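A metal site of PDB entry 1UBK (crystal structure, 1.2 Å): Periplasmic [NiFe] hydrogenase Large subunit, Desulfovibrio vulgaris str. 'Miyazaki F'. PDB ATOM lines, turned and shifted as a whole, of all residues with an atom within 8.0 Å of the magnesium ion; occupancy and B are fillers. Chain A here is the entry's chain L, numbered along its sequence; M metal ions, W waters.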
ATOM      1  N   PHE A  40      24.630 -14.336  21.971  1.00  0.00           N
ATOM      2  CA  PHE A  40      23.757 -13.483  21.188  1.00  0.00           C
ATOM      3  C   PHE A  40      22.353 -14.077  21.186  1.00  0.00           C
ATOM      4  O   PHE A  40      22.153 -15.289  21.073  1.00  0.00           O
ATOM      5  CB  PHE A  40      24.310 -13.409  19.741  1.00  0.00           C
ATOM      6  CG  PHE A  40      23.424 -12.680  18.762  1.00  0.00           C
ATOM      7  CD1 PHE A  40      23.477 -11.297  18.723  1.00  0.00           C
ATOM      8  CD2 PHE A  40      22.572 -13.394  17.908  1.00  0.00           C
ATOM      9  CE1 PHE A  40      22.685 -10.594  17.803  1.00  0.00           C
ATOM     10  CE2 PHE A  40      21.771 -12.700  16.982  1.00  0.00           C
ATOM     11  CZ  PHE A  40      21.849 -11.303  16.935  1.00  0.00           C
ATOM     12  N   GLU A  44      16.606  -7.500  18.443  1.00  0.00           N
ATOM     13  CA  GLU A  44      16.318  -6.476  17.434  1.00  0.00           C
ATOM     14  C   GLU A  44      15.802  -7.131  16.153  1.00  0.00           C
ATOM     15  O   GLU A  44      14.930  -6.568  15.484  1.00  0.00           O
ATOM     16  CB  GLU A  44      17.559  -5.640  17.135  1.00  0.00           C
ATOM     17  CG  GLU A  44      17.943  -4.728  18.324  1.00  0.00           C
ATOM     18  CD  GLU A  44      19.425  -4.415  18.355  1.00  0.00           C
ATOM     19  OE1 GLU A  44      20.240  -5.207  17.742  1.00  0.00           O
ATOM     20  OE2 GLU A  44      19.792  -3.457  19.034  1.00  0.00           O
ATOM     21  N   GLU A 319      27.334   2.927  16.302  1.00  0.00           N
ATOM     22  CA  GLU A 319      27.723   1.625  16.837  1.00  0.00           C
ATOM     23  C   GLU A 319      28.584   0.917  15.794  1.00  0.00           C
ATOM     24  O   GLU A 319      28.116   0.623  14.694  1.00  0.00           O
ATOM     25  CB  GLU A 319      26.516   0.752  17.215  1.00  0.00           C
ATOM     26  CG  GLU A 319      25.737   1.353  18.397  1.00  0.00           C
ATOM     27  CD  GLU A 319      24.647   0.354  18.800  1.00  0.00           C
ATOM     28  OE1 GLU A 319      24.872  -0.314  19.814  1.00  0.00           O
ATOM     29  OE2 GLU A 319      23.652   0.249  18.021  1.00  0.00           O
ATOM     30  N   TYR A 326      29.457  -9.272  13.415  1.00  0.00           N
ATOM     31  CA  TYR A 326      28.377  -8.796  12.533  1.00  0.00           C
ATOM     32  C   TYR A 326      29.019  -8.560  11.175  1.00  0.00           C
ATOM     33  O   TYR A 326      30.245  -8.491  11.042  1.00  0.00           O
ATOM     34  CB  TYR A 326      27.689  -7.486  13.025  1.00  0.00           C
ATOM     35  CG  TYR A 326      27.087  -7.740  14.399  1.00  0.00           C
ATOM     36  CD1 TYR A 326      27.778  -7.367  15.561  1.00  0.00           C
ATOM     37  CD2 TYR A 326      25.841  -8.359  14.475  1.00  0.00           C
ATOM     38  CE1 TYR A 326      27.169  -7.638  16.802  1.00  0.00           C
ATOM     39  CE2 TYR A 326      25.257  -8.611  15.717  1.00  0.00           C
ATOM     40  CZ  TYR A 326      25.942  -8.242  16.848  1.00  0.00           C
ATOM     41  OH  TYR A 326      25.371  -8.501  18.081  1.00  0.00           O
ATOM     42  N   PRO A 334      21.931   4.575  15.453  1.00  0.00           N
ATOM     43  CA  PRO A 334      20.874   3.567  15.673  1.00  0.00           C
ATOM     44  C   PRO A 334      19.574   3.763  14.902  1.00  0.00           C
ATOM     45  O   PRO A 334      18.898   2.753  14.719  1.00  0.00           O
ATOM     46  CB  PRO A 334      20.619   3.586  17.215  1.00  0.00           C
ATOM     47  CG  PRO A 334      21.542   4.585  17.748  1.00  0.00           C
ATOM     48  CD  PRO A 334      22.410   5.186  16.689  1.00  0.00           C
ATOM     49  N   GLY A 337      20.348   1.603  12.219  1.00  0.00           N
ATOM     50  CA  GLY A 337      21.133   0.495  12.735  1.00  0.00           C
ATOM     51  C   GLY A 337      20.902  -0.790  11.958  1.00  0.00           C
ATOM     52  O   GLY A 337      19.892  -0.959  11.240  1.00  0.00           O
ATOM     53  N   GLN A 338      21.839  -1.712  12.114  1.00  0.00           N
ATOM     54  CA  GLN A 338      21.827  -3.009  11.438  1.00  0.00           C
ATOM     55  C   GLN A 338      22.262  -4.093  12.421  1.00  0.00           C
ATOM     56  O   GLN A 338      23.229  -3.853  13.134  1.00  0.00           O
ATOM     57  CB  GLN A 338      22.808  -3.059  10.248  1.00  0.00           C
ATOM     58  CG  GLN A 338      22.403  -2.056   9.167  1.00  0.00           C
ATOM     59  CD  GLN A 338      23.397  -2.179   7.997  1.00  0.00           C
ATOM     60  OE1 GLN A 338      22.971  -2.419   6.861  1.00  0.00           O
ATOM     61  NE2 GLN A 338      24.677  -2.026   8.315  1.00  0.00           N
ATOM     62  N   THR A 339      21.577  -5.226  12.401  1.00  0.00           N
ATOM     63  CA  THR A 339      21.966  -6.332  13.310  1.00  0.00           C
ATOM     64  C   THR A 339      22.013  -7.587  12.438  1.00  0.00           C
ATOM     65  O   THR A 339      21.014  -8.276  12.246  1.00  0.00           O
ATOM     66  CB  THR A 339      20.981  -6.442  14.459  1.00  0.00           C
ATOM     67  OG1 THR A 339      20.982  -5.169  15.091  1.00  0.00           O
ATOM     68  CG2 THR A 339      21.495  -7.494  15.446  1.00  0.00           C
ATOM     69  N   TRP A 354      30.098 -10.461  20.617  1.00  0.00           N
ATOM     70  CA  TRP A 354      28.736 -10.211  20.099  1.00  0.00           C
ATOM     71  C   TRP A 354      28.271  -8.792  20.434  1.00  0.00           C
ATOM     72  O   TRP A 354      27.188  -8.412  19.942  1.00  0.00           O
ATOM     73  CB  TRP A 354      27.710 -11.227  20.637  1.00  0.00           C
ATOM     74  CG  TRP A 354      27.871 -12.588  20.012  1.00  0.00           C
ATOM     75  CD1 TRP A 354      28.339 -13.746  20.611  1.00  0.00           C
ATOM     76  CD2 TRP A 354      27.573 -12.976  18.659  1.00  0.00           C
ATOM     77  NE1 TRP A 354      28.339 -14.808  19.758  1.00  0.00           N
ATOM     78  CE2 TRP A 354      27.881 -14.351  18.522  1.00  0.00           C
ATOM     79  CE3 TRP A 354      27.078 -12.223  17.592  1.00  0.00           C
ATOM     80  CZ2 TRP A 354      27.682 -15.008  17.289  1.00  0.00           C
ATOM     81  CZ3 TRP A 354      26.888 -12.866  16.375  1.00  0.00           C
ATOM     82  CH2 TRP A 354      27.195 -14.243  16.271  1.00  0.00           C
ATOM     83  N   MET A 355      28.971  -8.017  21.260  1.00  0.00           N
ATOM     84  CA  MET A 355      28.534  -6.632  21.423  1.00  0.00           C
ATOM     85  C   MET A 355      29.028  -5.795  20.263  1.00  0.00           C
ATOM     86  O   MET A 355      30.131  -5.983  19.789  1.00  0.00           O
ATOM     87  CB  MET A 355      29.131  -6.037  22.702  1.00  0.00           C
ATOM     88  CG  MET A 355      28.436  -6.574  23.974  1.00  0.00           C
ATOM     89  SD  MET A 355      28.904  -5.443  25.347  1.00  0.00           S
ATOM     90  CE  MET A 355      28.563  -6.510  26.761  1.00  0.00           C
ATOM     91  N   LYS A 356      28.194  -4.837  19.847  1.00  0.00           N
ATOM     92  CA  LYS A 356      28.648  -3.729  19.030  1.00  0.00           C
ATOM     93  C   LYS A 356      29.504  -2.789  19.897  1.00  0.00           C
ATOM     94  O   LYS A 356      29.531  -2.923  21.129  1.00  0.00           O
ATOM     95  CB  LYS A 356      27.489  -2.971  18.425  1.00  0.00           C
ATOM     96  CG  LYS A 356      26.594  -3.860  17.528  1.00  0.00           C
ATOM     97  CD  LYS A 356      25.385  -3.052  17.013  1.00  0.00           C
ATOM     98  CE  LYS A 356      24.477  -3.959  16.157  1.00  0.00           C
ATOM     99  NZ  LYS A 356      23.163  -3.264  15.903  1.00  0.00           N
ATOM    100  N   PRO A 358      29.759   1.023  20.658  1.00  0.00           N
ATOM    101  CA  PRO A 358      29.218   2.385  20.521  1.00  0.00           C
ATOM    102  C   PRO A 358      30.352   3.380  20.759  1.00  0.00           C
ATOM    103  O   PRO A 358      31.165   3.225  21.661  1.00  0.00           O
ATOM    104  CB  PRO A 358      28.143   2.487  21.585  1.00  0.00           C
ATOM    105  CG  PRO A 358      27.890   1.073  22.041  1.00  0.00           C
ATOM    106  CD  PRO A 358      29.253   0.384  21.887  1.00  0.00           C
ATOM    107  N   SER A 465      19.381   3.644  25.594  1.00  0.00           N
ATOM    108  CA  SER A 465      18.508   4.289  24.574  1.00  0.00           C
ATOM    109  C   SER A 465      17.931   3.198  23.702  1.00  0.00           C
ATOM    110  O   SER A 465      18.624   2.268  23.286  1.00  0.00           O
ATOM    111  CB  SER A 465      19.256   5.397  23.817  1.00  0.00           C
ATOM    112  OG  SER A 465      20.460   4.943  23.201  1.00  0.00           O
ATOM    113  N   TRP A 467      15.555   2.940  20.138  1.00  0.00           N
ATOM    114  CA  TRP A 467      15.344   3.749  18.932  1.00  0.00           C
ATOM    115  C   TRP A 467      14.398   3.025  17.990  1.00  0.00           C
ATOM    116  O   TRP A 467      14.745   1.900  17.601  1.00  0.00           O
ATOM    117  CB  TRP A 467      16.696   3.921  18.236  1.00  0.00           C
ATOM    118  CG  TRP A 467      17.798   4.546  19.070  1.00  0.00           C
ATOM    119  CD1 TRP A 467      18.535   3.899  20.034  1.00  0.00           C
ATOM    120  CD2 TRP A 467      18.257   5.900  19.009  1.00  0.00           C
ATOM    121  NE1 TRP A 467      19.445   4.835  20.561  1.00  0.00           N
ATOM    122  CE2 TRP A 467      19.300   6.054  19.961  1.00  0.00           C
ATOM    123  CE3 TRP A 467      17.893   7.010  18.229  1.00  0.00           C
ATOM    124  CZ2 TRP A 467      19.980   7.260  20.179  1.00  0.00           C
ATOM    125  CZ3 TRP A 467      18.549   8.202  18.421  1.00  0.00           C
ATOM    126  CH2 TRP A 467      19.572   8.326  19.365  1.00  0.00           C
ATOM    127  N   PHE A 478      14.159  -1.415  15.078  1.00  0.00           N
ATOM    128  CA  PHE A 478      14.202  -1.130  16.500  1.00  0.00           C
ATOM    129  C   PHE A 478      15.637  -1.458  16.949  1.00  0.00           C
ATOM    130  O   PHE A 478      16.118  -2.579  16.726  1.00  0.00           O
ATOM    131  CB  PHE A 478      13.193  -2.006  17.238  1.00  0.00           C
ATOM    132  CG  PHE A 478      12.851  -1.425  18.633  1.00  0.00           C
ATOM    133  CD1 PHE A 478      13.777  -1.537  19.672  1.00  0.00           C
ATOM    134  CD2 PHE A 478      11.640  -0.790  18.834  1.00  0.00           C
ATOM    135  CE1 PHE A 478      13.459  -0.968  20.928  1.00  0.00           C
ATOM    136  CE2 PHE A 478      11.311  -0.245  20.046  1.00  0.00           C
ATOM    137  CZ  PHE A 478      12.225  -0.346  21.104  1.00  0.00           C
ATOM    138  N   GLN A 479      16.291  -0.485  17.574  1.00  0.00           N
ATOM    139  CA  GLN A 479      17.691  -0.713  17.982  1.00  0.00           C
ATOM    140  C   GLN A 479      17.813  -0.356  19.445  1.00  0.00           C
ATOM    141  O   GLN A 479      17.380   0.715  19.884  1.00  0.00           O
ATOM    142  CB  GLN A 479      18.657   0.113  17.126  1.00  0.00           C
ATOM    143  CG  GLN A 479      18.681  -0.309  15.661  1.00  0.00           C
ATOM    144  CD  GLN A 479      19.386  -1.632  15.434  1.00  0.00           C
ATOM    145  OE1 GLN A 479      20.360  -1.952  16.114  1.00  0.00           O
ATOM    146  NE2 GLN A 479      18.967  -2.403  14.438  1.00  0.00           N
ATOM    147  N   LEU A 480      18.470  -1.247  20.191  1.00  0.00           N
ATOM    148  CA  LEU A 480      18.837  -0.940  21.575  1.00  0.00           C
ATOM    149  C   LEU A 480      20.320  -0.611  21.642  1.00  0.00           C
ATOM    150  O   LEU A 480      21.113  -1.331  21.055  1.00  0.00           O
ATOM    151  CB  LEU A 480      18.587  -2.124  22.520  1.00  0.00           C
ATOM    152  CG  LEU A 480      17.173  -2.640  22.671  1.00  0.00           C
ATOM    153  CD1 LEU A 480      16.618  -3.332  21.463  1.00  0.00           C
ATOM    154  CD2 LEU A 480      17.138  -3.623  23.877  1.00  0.00           C
ATOM    155  N   VAL A 481      20.670   0.473  22.346  1.00  0.00           N
ATOM    156  CA  VAL A 481      22.070   0.810  22.588  1.00  0.00           C
ATOM    157  C   VAL A 481      22.171   0.869  24.115  1.00  0.00           C
ATOM    158  O   VAL A 481      21.500   1.755  24.711  1.00  0.00           O
ATOM    159  CB  VAL A 481      22.484   2.136  21.976  1.00  0.00           C
ATOM    160  CG1 VAL A 481      23.982   2.315  22.194  1.00  0.00           C
ATOM    161  CG2 VAL A 481      22.108   2.151  20.477  1.00  0.00           C
ATOM    162  N   VAL A 482      22.859  -0.098  24.740  1.00  0.00           N
ATOM    163  CA  VAL A 482      22.624  -0.317  26.165  1.00  0.00           C
ATOM    164  C   VAL A 482      23.877   0.057  26.934  1.00  0.00           C
ATOM    165  O   VAL A 482      24.995   0.062  26.366  1.00  0.00           O
ATOM    166  CB  VAL A 482      22.221  -1.798  26.321  1.00  0.00           C
ATOM    167  CG1 VAL A 482      21.793  -2.180  27.707  1.00  0.00           C
ATOM    168  CG2 VAL A 482      21.042  -2.117  25.393  1.00  0.00           C
ATOM    169  N   THR A 485      26.857  -2.056  26.587  1.00  0.00           N
ATOM    170  CA  THR A 485      27.408  -2.013  25.230  1.00  0.00           C
ATOM    171  C   THR A 485      28.490  -0.932  25.152  1.00  0.00           C
ATOM    172  O   THR A 485      29.586  -1.128  24.638  1.00  0.00           O
ATOM    173  CB  THR A 485      26.300  -1.699  24.180  1.00  0.00           C
ATOM    174  OG1 THR A 485      25.068  -2.359  24.490  1.00  0.00           O
ATOM    175  CG2 THR A 485      26.803  -2.131  22.810  1.00  0.00           C
ATOM    176  N   CYS A 531      22.146  -7.437  28.541  1.00  0.00           N
ATOM    177  CA  CYS A 531      21.969  -6.058  28.179  1.00  0.00           C
ATOM    178  C   CYS A 531      22.861  -5.666  27.034  1.00  0.00           C
ATOM    179  O   CYS A 531      22.411  -5.071  26.043  1.00  0.00           O
ATOM    180  CB  CYS A 531      22.274  -5.146  29.384  1.00  0.00           C
ATOM    181  SG  CYS A 531      20.835  -4.824  30.386  1.00  0.00           S
ATOM    182  N   GLY A 532      24.149  -5.961  27.108  1.00  0.00           N
ATOM    183  CA  GLY A 532      25.079  -5.398  26.138  1.00  0.00           C
ATOM    184  C   GLY A 532      24.824  -5.895  24.720  1.00  0.00           C
ATOM    185  O   GLY A 532      25.013  -5.138  23.776  1.00  0.00           O
ATOM    186  N   VAL A 533      24.469  -7.160  24.585  1.00  0.00           N
ATOM    187  CA  VAL A 533      24.304  -7.800  23.300  1.00  0.00           C
ATOM    188  C   VAL A 533      22.876  -7.889  22.822  1.00  0.00           C
ATOM    189  O   VAL A 533      22.596  -7.614  21.620  1.00  0.00           O
ATOM    190  CB  VAL A 533      24.828  -9.259  23.317  1.00  0.00           C
ATOM    191  CG1 VAL A 533      24.582  -9.917  21.968  1.00  0.00           C
ATOM    192  CG2 VAL A 533      26.255  -9.361  23.702  1.00  0.00           C
ATOM    193  N   HIS A 534      21.910  -8.191  23.704  1.00  0.00           N
ATOM    194  CA  HIS A 534      20.516  -8.378  23.342  1.00  0.00           C
ATOM    195  C   HIS A 534      20.392  -9.264  22.072  1.00  0.00           C
ATOM    196  O   HIS A 534      21.071 -10.310  22.012  1.00  0.00           O
ATOM    197  CB  HIS A 534      19.751  -7.037  23.292  1.00  0.00           C
ATOM    198  CG  HIS A 534      20.439  -5.877  22.712  1.00  0.00           C
ATOM    199  ND1 HIS A 534      21.428  -5.192  23.407  1.00  0.00           N
ATOM    200  CD2 HIS A 534      20.458  -5.354  21.474  1.00  0.00           C
ATOM    201  CE1 HIS A 534      21.943  -4.268  22.634  1.00  0.00           C
ATOM    202  NE2 HIS A 534      21.353  -4.333  21.454  1.00  0.00           N
ATOM    203  OXT HIS A 534      19.535  -8.937  21.198  1.00  0.00           O
HETATM  204 MG    MG M   1      21.753  -2.948  19.825  1.00  0.00          MG
HETATM  205  O   HOH W   1      22.567  -4.455  18.626  1.00  0.00           O
HETATM  206  O   HOH W   2      21.988  -1.688  18.238  1.00  0.00           O
HETATM  207  O   HOH W   3      23.698  -2.525  20.555  1.00  0.00           O
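The backbone carbonyl oxygen (O) of Cys 531 lies within hydrogen-bond range of a ring nitrogen (ND1) of His 534. OE2 of Glu 44 sits close to OE1 of Gln 479 (3.3 Å). OE1 of Glu 44 is in hydrogen-bond range of OG1 of Thr 339 (2.8 Å). The side-chain carboxylate (OE1) of Glu 44 is in salt-bridge range of the side-chain amino group (NZ) of Lys 356, 3.96 Å away.
Water W2 binds the magnesium ion (2.0 Å). Water W1 binds the magnesium ion (2.1 Å). Water W3 is bound to the magnesium ion (2.1 Å). O of Leu 480 is bound to the magnesium ion (2.1 Å). The side-chain carboxylate (OE2) of Glu 44 binds the magnesium ion, 2.2 Å away. NE2 of His 534 binds the magnesium ion, at 2.2 Å.
Within 4 Å of the magnesium ion: Glu 44, Leu 480 and His 534. The nearest printed residue that does not touch the magnesium ion is Glu 319 (4.1 Å).
Water W1 bridges OE1 of Glu 44 (2.6 Å) and NZ of Lys 356 (3.0 Å). Water W2 lies within hydrogen-bond range of OE2 of Glu 319 (2.6 Å), OE1 of Gln 479 (2.7 Å) and NZ of Lys 356 (3.1 Å).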
